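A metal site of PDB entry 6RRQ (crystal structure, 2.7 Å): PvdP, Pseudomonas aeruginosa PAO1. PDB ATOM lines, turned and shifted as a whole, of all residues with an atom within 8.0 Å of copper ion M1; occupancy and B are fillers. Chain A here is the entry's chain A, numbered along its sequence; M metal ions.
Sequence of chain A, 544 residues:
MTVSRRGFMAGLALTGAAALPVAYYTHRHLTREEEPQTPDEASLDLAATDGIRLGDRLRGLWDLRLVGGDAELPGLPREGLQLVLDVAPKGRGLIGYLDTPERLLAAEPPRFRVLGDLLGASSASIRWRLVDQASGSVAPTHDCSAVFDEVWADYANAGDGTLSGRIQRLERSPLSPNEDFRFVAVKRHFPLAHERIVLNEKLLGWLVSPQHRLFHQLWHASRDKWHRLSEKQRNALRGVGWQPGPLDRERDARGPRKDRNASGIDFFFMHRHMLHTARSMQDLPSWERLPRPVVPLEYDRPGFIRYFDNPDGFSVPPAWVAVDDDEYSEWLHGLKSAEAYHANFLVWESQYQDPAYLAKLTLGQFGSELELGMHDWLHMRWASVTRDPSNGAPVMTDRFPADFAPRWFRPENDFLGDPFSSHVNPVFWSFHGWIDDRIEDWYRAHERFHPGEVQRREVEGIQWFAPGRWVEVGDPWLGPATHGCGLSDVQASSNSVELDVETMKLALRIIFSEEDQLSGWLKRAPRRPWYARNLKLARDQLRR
ND1 of His 216 lies within hydrogen-bond range of O of Pro 419 (2.8 Å). A ring nitrogen (ND1) of His 216 sits at hydrogen-bond distance from a ring nitrogen (ND1) of His 423 (2.8 Å). ND1 of His 271 sits at hydrogen-bond distance from O of Phe 267, at 2.8 Å.
Of the 20 residues printed, 3 come within 4 Å of copper ion M1. Along chain A the residues within 4 Å of copper ion M1 span positions 216 to 271. The nearest printed residue that does not touch copper ion M1 is Met 270 (4.1 Å).
Copper ion M1 is bound by a ring nitrogen (NE2) of His 216 (2.1 Å), a ring nitrogen (NE2) of His 271 (2.2 Å) and a ring nitrogen (NE2) of His 220 (2.3 Å). Copper ion M1 has three donor atoms within binding distance.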
ATOM      1  N   PHE A 215     -13.852  13.601  -4.931  1.00  0.00           N
ATOM      2  CA  PHE A 215     -13.202  13.568  -3.641  1.00  0.00           C
ATOM      3  C   PHE A 215     -13.142  14.996  -3.105  1.00  0.00           C
ATOM      4  O   PHE A 215     -13.658  15.294  -2.019  1.00  0.00           O
ATOM      5  CB  PHE A 215     -11.784  12.959  -3.726  1.00  0.00           C
ATOM      6  CG  PHE A 215     -10.970  13.133  -2.456  1.00  0.00           C
ATOM      7  CD1 PHE A 215     -10.199  14.282  -2.243  1.00  0.00           C
ATOM      8  CD2 PHE A 215     -10.989  12.168  -1.466  1.00  0.00           C
ATOM      9  CE1 PHE A 215      -9.487  14.457  -1.068  1.00  0.00           C
ATOM     10  CE2 PHE A 215     -10.264  12.340  -0.287  1.00  0.00           C
ATOM     11  CZ  PHE A 215      -9.515  13.475  -0.089  1.00  0.00           C
ATOM     12  N   HIS A 216     -12.534  15.884  -3.892  1.00  0.00           N
ATOM     13  CA  HIS A 216     -12.344  17.273  -3.484  1.00  0.00           C
ATOM     14  C   HIS A 216     -13.677  17.941  -3.106  1.00  0.00           C
ATOM     15  O   HIS A 216     -13.787  18.560  -2.008  1.00  0.00           O
ATOM     16  CB  HIS A 216     -11.654  18.044  -4.603  1.00  0.00           C
ATOM     17  CG  HIS A 216     -10.945  19.288  -4.157  1.00  0.00           C
ATOM     18  ND1 HIS A 216     -10.459  20.222  -5.041  1.00  0.00           N
ATOM     19  CD2 HIS A 216     -10.622  19.735  -2.922  1.00  0.00           C
ATOM     20  CE1 HIS A 216      -9.862  21.192  -4.375  1.00  0.00           C
ATOM     21  NE2 HIS A 216      -9.961  20.922  -3.084  1.00  0.00           N
ATOM     22  N   GLN A 217     -14.681  17.792  -3.971  1.00  0.00           N
ATOM     23  CA  GLN A 217     -16.008  18.347  -3.681  1.00  0.00           C
ATOM     24  C   GLN A 217     -16.622  17.826  -2.382  1.00  0.00           C
ATOM     25  O   GLN A 217     -17.117  18.615  -1.556  1.00  0.00           O
ATOM     26  CB  GLN A 217     -17.000  18.098  -4.822  1.00  0.00           C
ATOM     27  CG  GLN A 217     -18.199  19.049  -4.768  1.00  0.00           C
ATOM     28  CD  GLN A 217     -19.323  18.645  -5.707  1.00  0.00           C
ATOM     29  OE1 GLN A 217     -20.464  19.032  -5.503  1.00  0.00           O
ATOM     30  NE2 GLN A 217     -18.995  17.861  -6.720  1.00  0.00           N
ATOM     31  N   TRP A 219     -15.092  16.183   0.224  1.00  0.00           N
ATOM     32  CA  TRP A 219     -14.236  16.592   1.362  1.00  0.00           C
ATOM     33  C   TRP A 219     -14.627  17.979   1.931  1.00  0.00           C
ATOM     34  O   TRP A 219     -14.744  18.143   3.147  1.00  0.00           O
ATOM     35  CB  TRP A 219     -12.758  16.623   0.915  1.00  0.00           C
ATOM     36  CG  TRP A 219     -11.831  16.755   2.029  1.00  0.00           C
ATOM     37  CD1 TRP A 219     -11.265  15.754   2.752  1.00  0.00           C
ATOM     38  CD2 TRP A 219     -11.353  17.967   2.585  1.00  0.00           C
ATOM     39  NE1 TRP A 219     -10.467  16.255   3.733  1.00  0.00           N
ATOM     40  CE2 TRP A 219     -10.509  17.626   3.670  1.00  0.00           C
ATOM     41  CE3 TRP A 219     -11.554  19.326   2.292  1.00  0.00           C
ATOM     42  CZ2 TRP A 219      -9.866  18.585   4.436  1.00  0.00           C
ATOM     43  CZ3 TRP A 219     -10.913  20.275   3.057  1.00  0.00           C
ATOM     44  CH2 TRP A 219     -10.090  19.898   4.134  1.00  0.00           C
ATOM     45  N   HIS A 220     -14.810  18.968   1.049  1.00  0.00           N
ATOM     46  CA  HIS A 220     -15.287  20.302   1.443  1.00  0.00           C
ATOM     47  C   HIS A 220     -16.746  20.262   1.843  1.00  0.00           C
ATOM     48  O   HIS A 220     -17.121  20.787   2.868  1.00  0.00           O
ATOM     49  CB  HIS A 220     -15.085  21.321   0.318  1.00  0.00           C
ATOM     50  CG  HIS A 220     -13.668  21.757   0.164  1.00  0.00           C
ATOM     51  ND1 HIS A 220     -13.009  22.470   1.144  1.00  0.00           N
ATOM     52  CD2 HIS A 220     -12.771  21.560  -0.830  1.00  0.00           C
ATOM     53  CE1 HIS A 220     -11.764  22.706   0.736  1.00  0.00           C
ATOM     54  NE2 HIS A 220     -11.601  22.159  -0.445  1.00  0.00           N
ATOM     55  N   ARG A 223     -17.279  18.762   5.534  1.00  0.00           N
ATOM     56  CA  ARG A 223     -16.836  19.626   6.613  1.00  0.00           C
ATOM     57  C   ARG A 223     -17.546  20.966   6.590  1.00  0.00           C
ATOM     58  O   ARG A 223     -17.976  21.443   7.669  1.00  0.00           O
ATOM     59  CB  ARG A 223     -15.320  19.772   6.664  1.00  0.00           C
ATOM     60  CG  ARG A 223     -14.692  20.411   5.466  1.00  0.00           C
ATOM     61  CD  ARG A 223     -13.219  20.047   5.386  1.00  0.00           C
ATOM     62  NE  ARG A 223     -12.476  20.493   6.561  1.00  0.00           N
ATOM     63  CZ  ARG A 223     -12.021  21.734   6.773  1.00  0.00           C
ATOM     64  NH1 ARG A 223     -12.199  22.703   5.884  1.00  0.00           N
ATOM     65  NH2 ARG A 223     -11.360  22.009   7.883  1.00  0.00           N
ATOM     66  N   PHE A 267      -7.739  21.178   6.967  1.00  0.00           N
ATOM     67  CA  PHE A 267      -7.548  22.049   5.813  1.00  0.00           C
ATOM     68  C   PHE A 267      -6.080  22.159   5.413  1.00  0.00           C
ATOM     69  O   PHE A 267      -5.733  21.914   4.247  1.00  0.00           O
ATOM     70  CB  PHE A 267      -8.152  23.433   6.080  1.00  0.00           C
ATOM     71  CG  PHE A 267      -7.614  24.495   5.161  1.00  0.00           C
ATOM     72  CD1 PHE A 267      -8.041  24.561   3.848  1.00  0.00           C
ATOM     73  CD2 PHE A 267      -6.665  25.406   5.604  1.00  0.00           C
ATOM     74  CE1 PHE A 267      -7.521  25.515   2.997  1.00  0.00           C
ATOM     75  CE2 PHE A 267      -6.149  26.359   4.767  1.00  0.00           C
ATOM     76  CZ  PHE A 267      -6.585  26.426   3.459  1.00  0.00           C
ATOM     77  N   MET A 270      -4.598  18.526   4.405  1.00  0.00           N
ATOM     78  CA  MET A 270      -5.158  17.916   3.195  1.00  0.00           C
ATOM     79  C   MET A 270      -4.545  18.512   1.960  1.00  0.00           C
ATOM     80  O   MET A 270      -4.099  17.789   1.096  1.00  0.00           O
ATOM     81  CB  MET A 270      -6.669  18.030   3.121  1.00  0.00           C
ATOM     82  CG  MET A 270      -7.277  17.100   2.072  1.00  0.00           C
ATOM     83  SD  MET A 270      -7.154  17.723   0.394  1.00  0.00           S
ATOM     84  CE  MET A 270      -8.707  18.597   0.219  1.00  0.00           C
ATOM     85  N   HIS A 271      -4.519  19.843   1.862  1.00  0.00           N
ATOM     86  CA  HIS A 271      -3.971  20.487   0.664  1.00  0.00           C
ATOM     87  C   HIS A 271      -2.463  20.307   0.548  1.00  0.00           C
ATOM     88  O   HIS A 271      -1.960  20.304  -0.578  1.00  0.00           O
ATOM     89  CB  HIS A 271      -4.372  21.954   0.626  1.00  0.00           C
ATOM     90  CG  HIS A 271      -5.846  22.139   0.502  1.00  0.00           C
ATOM     91  ND1 HIS A 271      -6.664  22.277   1.601  1.00  0.00           N
ATOM     92  CD2 HIS A 271      -6.660  22.094  -0.575  1.00  0.00           C
ATOM     93  CE1 HIS A 271      -7.921  22.365   1.192  1.00  0.00           C
ATOM     94  NE2 HIS A 271      -7.950  22.241  -0.121  1.00  0.00           N
ATOM     95  N   MET A 274      -2.225  17.108  -1.193  1.00  0.00           N
ATOM     96  CA  MET A 274      -2.547  17.290  -2.609  1.00  0.00           C
ATOM     97  C   MET A 274      -1.387  17.964  -3.346  1.00  0.00           C
ATOM     98  O   MET A 274      -1.128  17.685  -4.517  1.00  0.00           O
ATOM     99  CB  MET A 274      -3.831  18.098  -2.751  1.00  0.00           C
ATOM    100  CG  MET A 274      -4.580  17.791  -4.042  1.00  0.00           C
ATOM    101  SD  MET A 274      -5.939  18.932  -4.357  1.00  0.00           S
ATOM    102  CE  MET A 274      -6.896  18.605  -2.867  1.00  0.00           C
ATOM    103  N   GLU A 371      -8.315  29.651   6.008  1.00  0.00           N
ATOM    104  CA  GLU A 371      -9.277  29.063   5.063  1.00  0.00           C
ATOM    105  C   GLU A 371     -10.465  29.988   4.824  1.00  0.00           C
ATOM    106  O   GLU A 371     -10.849  30.267   3.700  1.00  0.00           O
ATOM    107  CB  GLU A 371      -9.815  27.714   5.504  1.00  0.00           C
ATOM    108  CG  GLU A 371     -10.552  27.005   4.369  1.00  0.00           C
ATOM    109  CD  GLU A 371     -11.230  25.709   4.760  1.00  0.00           C
ATOM    110  OE1 GLU A 371     -11.204  25.315   5.952  1.00  0.00           O
ATOM    111  OE2 GLU A 371     -11.792  25.085   3.828  1.00  0.00           O
ATOM    112  N   HIS A 375      -8.276  32.502   2.046  1.00  0.00           N
ATOM    113  CA  HIS A 375      -8.303  31.415   1.044  1.00  0.00           C
ATOM    114  C   HIS A 375      -9.513  31.455   0.129  1.00  0.00           C
ATOM    115  O   HIS A 375      -9.382  31.320  -1.089  1.00  0.00           O
ATOM    116  CB  HIS A 375      -8.207  30.046   1.733  1.00  0.00           C
ATOM    117  CG  HIS A 375      -8.622  28.901   0.877  1.00  0.00           C
ATOM    118  ND1 HIS A 375      -9.911  28.397   0.885  1.00  0.00           N
ATOM    119  CD2 HIS A 375      -7.935  28.168  -0.032  1.00  0.00           C
ATOM    120  CE1 HIS A 375      -9.989  27.405   0.016  1.00  0.00           C
ATOM    121  NE2 HIS A 375      -8.801  27.240  -0.549  1.00  0.00           N
ATOM    122  N   HIS A 379      -9.427  32.357  -4.144  1.00  0.00           N
ATOM    123  CA  HIS A 379     -10.170  31.605  -5.180  1.00  0.00           C
ATOM    124  C   HIS A 379     -10.978  32.503  -6.095  1.00  0.00           C
ATOM    125  O   HIS A 379     -10.770  32.504  -7.289  1.00  0.00           O
ATOM    126  CB  HIS A 379     -11.078  30.510  -4.566  1.00  0.00           C
ATOM    127  CG  HIS A 379     -10.394  29.203  -4.356  1.00  0.00           C
ATOM    128  ND1 HIS A 379     -10.720  28.063  -5.062  1.00  0.00           N
ATOM    129  CD2 HIS A 379      -9.386  28.863  -3.526  1.00  0.00           C
ATOM    130  CE1 HIS A 379      -9.941  27.084  -4.676  1.00  0.00           C
ATOM    131  NE2 HIS A 379      -9.110  27.535  -3.748  1.00  0.00           N
ATOM    132  N   ASP A 418     -15.620  26.400  -7.199  1.00  0.00           N
ATOM    133  CA  ASP A 418     -16.272  25.133  -6.909  1.00  0.00           C
ATOM    134  C   ASP A 418     -15.167  24.111  -6.752  1.00  0.00           C
ATOM    135  O   ASP A 418     -14.369  23.963  -7.667  1.00  0.00           O
ATOM    136  CB  ASP A 418     -17.181  24.802  -8.093  1.00  0.00           C
ATOM    137  CG  ASP A 418     -17.930  23.509  -7.942  1.00  0.00           C
ATOM    138  OD1 ASP A 418     -18.057  22.980  -6.825  1.00  0.00           O
ATOM    139  OD2 ASP A 418     -18.418  23.040  -8.996  1.00  0.00           O
ATOM    140  N   PRO A 419     -15.100  23.426  -5.592  1.00  0.00           N
ATOM    141  CA  PRO A 419     -14.002  22.477  -5.343  1.00  0.00           C
ATOM    142  C   PRO A 419     -13.975  21.222  -6.240  1.00  0.00           C
ATOM    143  O   PRO A 419     -12.945  20.553  -6.319  1.00  0.00           O
ATOM    144  CB  PRO A 419     -14.183  22.118  -3.875  1.00  0.00           C
ATOM    145  CG  PRO A 419     -15.633  22.379  -3.597  1.00  0.00           C
ATOM    146  CD  PRO A 419     -15.910  23.609  -4.369  1.00  0.00           C
ATOM    147  N   PHE A 420     -15.096  20.925  -6.898  1.00  0.00           N
ATOM    148  CA  PHE A 420     -15.209  19.948  -7.989  1.00  0.00           C
ATOM    149  C   PHE A 420     -14.346  20.309  -9.208  1.00  0.00           C
ATOM    150  O   PHE A 420     -13.924  19.411  -9.960  1.00  0.00           O
ATOM    151  CB  PHE A 420     -16.687  19.886  -8.427  1.00  0.00           C
ATOM    152  CG  PHE A 420     -16.978  18.928  -9.566  1.00  0.00           C
ATOM    153  CD1 PHE A 420     -17.204  17.566  -9.327  1.00  0.00           C
ATOM    154  CD2 PHE A 420     -17.084  19.385 -10.886  1.00  0.00           C
ATOM    155  CE1 PHE A 420     -17.495  16.697 -10.364  1.00  0.00           C
ATOM    156  CE2 PHE A 420     -17.365  18.515 -11.928  1.00  0.00           C
ATOM    157  CZ  PHE A 420     -17.579  17.168 -11.669  1.00  0.00           C
ATOM    158  N   SER A 422     -11.948  23.522  -8.954  1.00  0.00           N
ATOM    159  CA  SER A 422     -10.942  24.570  -8.698  1.00  0.00           C
ATOM    160  C   SER A 422      -9.493  24.096  -8.838  1.00  0.00           C
ATOM    161  O   SER A 422      -8.659  24.783  -9.437  1.00  0.00           O
ATOM    162  CB  SER A 422     -11.161  25.216  -7.334  1.00  0.00           C
ATOM    163  OG  SER A 422     -11.124  24.228  -6.323  1.00  0.00           O
ATOM    164  N   HIS A 423      -9.198  22.903  -8.301  1.00  0.00           N
ATOM    165  CA  HIS A 423      -7.878  22.227  -8.440  1.00  0.00           C
ATOM    166  C   HIS A 423      -7.343  22.029  -9.851  1.00  0.00           C
ATOM    167  O   HIS A 423      -6.168  21.713 -10.012  1.00  0.00           O
ATOM    168  CB  HIS A 423      -7.925  20.858  -7.776  1.00  0.00           C
ATOM    169  CG  HIS A 423      -8.962  19.939  -8.347  1.00  0.00           C
ATOM    170  ND1 HIS A 423     -10.243  19.896  -7.861  1.00  0.00           N
ATOM    171  CD2 HIS A 423      -8.908  19.055  -9.370  1.00  0.00           C
ATOM    172  CE1 HIS A 423     -10.952  19.036  -8.579  1.00  0.00           C
ATOM    173  NE2 HIS A 423     -10.153  18.498  -9.493  1.00  0.00           N
ATOM    174  N   PHE A 428      -4.549  28.017  -8.932  1.00  0.00           N
ATOM    175  CA  PHE A 428      -4.687  27.158  -7.711  1.00  0.00           C
ATOM    176  C   PHE A 428      -3.371  26.717  -7.031  1.00  0.00           C
ATOM    177  O   PHE A 428      -3.216  26.869  -5.807  1.00  0.00           O
ATOM    178  CB  PHE A 428      -5.480  25.899  -8.078  1.00  0.00           C
ATOM    179  CG  PHE A 428      -5.919  25.064  -6.916  1.00  0.00           C
ATOM    180  CD1 PHE A 428      -5.102  24.036  -6.434  1.00  0.00           C
ATOM    181  CD2 PHE A 428      -7.168  25.239  -6.338  1.00  0.00           C
ATOM    182  CE1 PHE A 428      -5.505  23.220  -5.394  1.00  0.00           C
ATOM    183  CE2 PHE A 428      -7.588  24.425  -5.287  1.00  0.00           C
ATOM    184  CZ  PHE A 428      -6.755  23.416  -4.822  1.00  0.00           C
ATOM    185  N   HIS A 432      -2.116  27.850  -3.337  1.00  0.00           N
ATOM    186  CA  HIS A 432      -2.070  26.789  -2.336  1.00  0.00           C
ATOM    187  C   HIS A 432      -0.631  26.501  -1.994  1.00  0.00           C
ATOM    188  O   HIS A 432      -0.347  26.167  -0.851  1.00  0.00           O
ATOM    189  CB  HIS A 432      -2.818  25.551  -2.770  1.00  0.00           C
ATOM    190  CG  HIS A 432      -4.277  25.624  -2.450  1.00  0.00           C
ATOM    191  ND1 HIS A 432      -4.752  25.468  -1.166  1.00  0.00           N
ATOM    192  CD2 HIS A 432      -5.348  25.899  -3.235  1.00  0.00           C
ATOM    193  CE1 HIS A 432      -6.063  25.608  -1.182  1.00  0.00           C
ATOM    194  NE2 HIS A 432      -6.454  25.893  -2.418  1.00  0.00           N
HETATM  195 CU    CU M   1      -9.602  22.231  -1.502  1.00  0.00          CU
HETATM  196 CU    CU M   2      -8.372  26.091  -2.149  1.00  0.00          CU
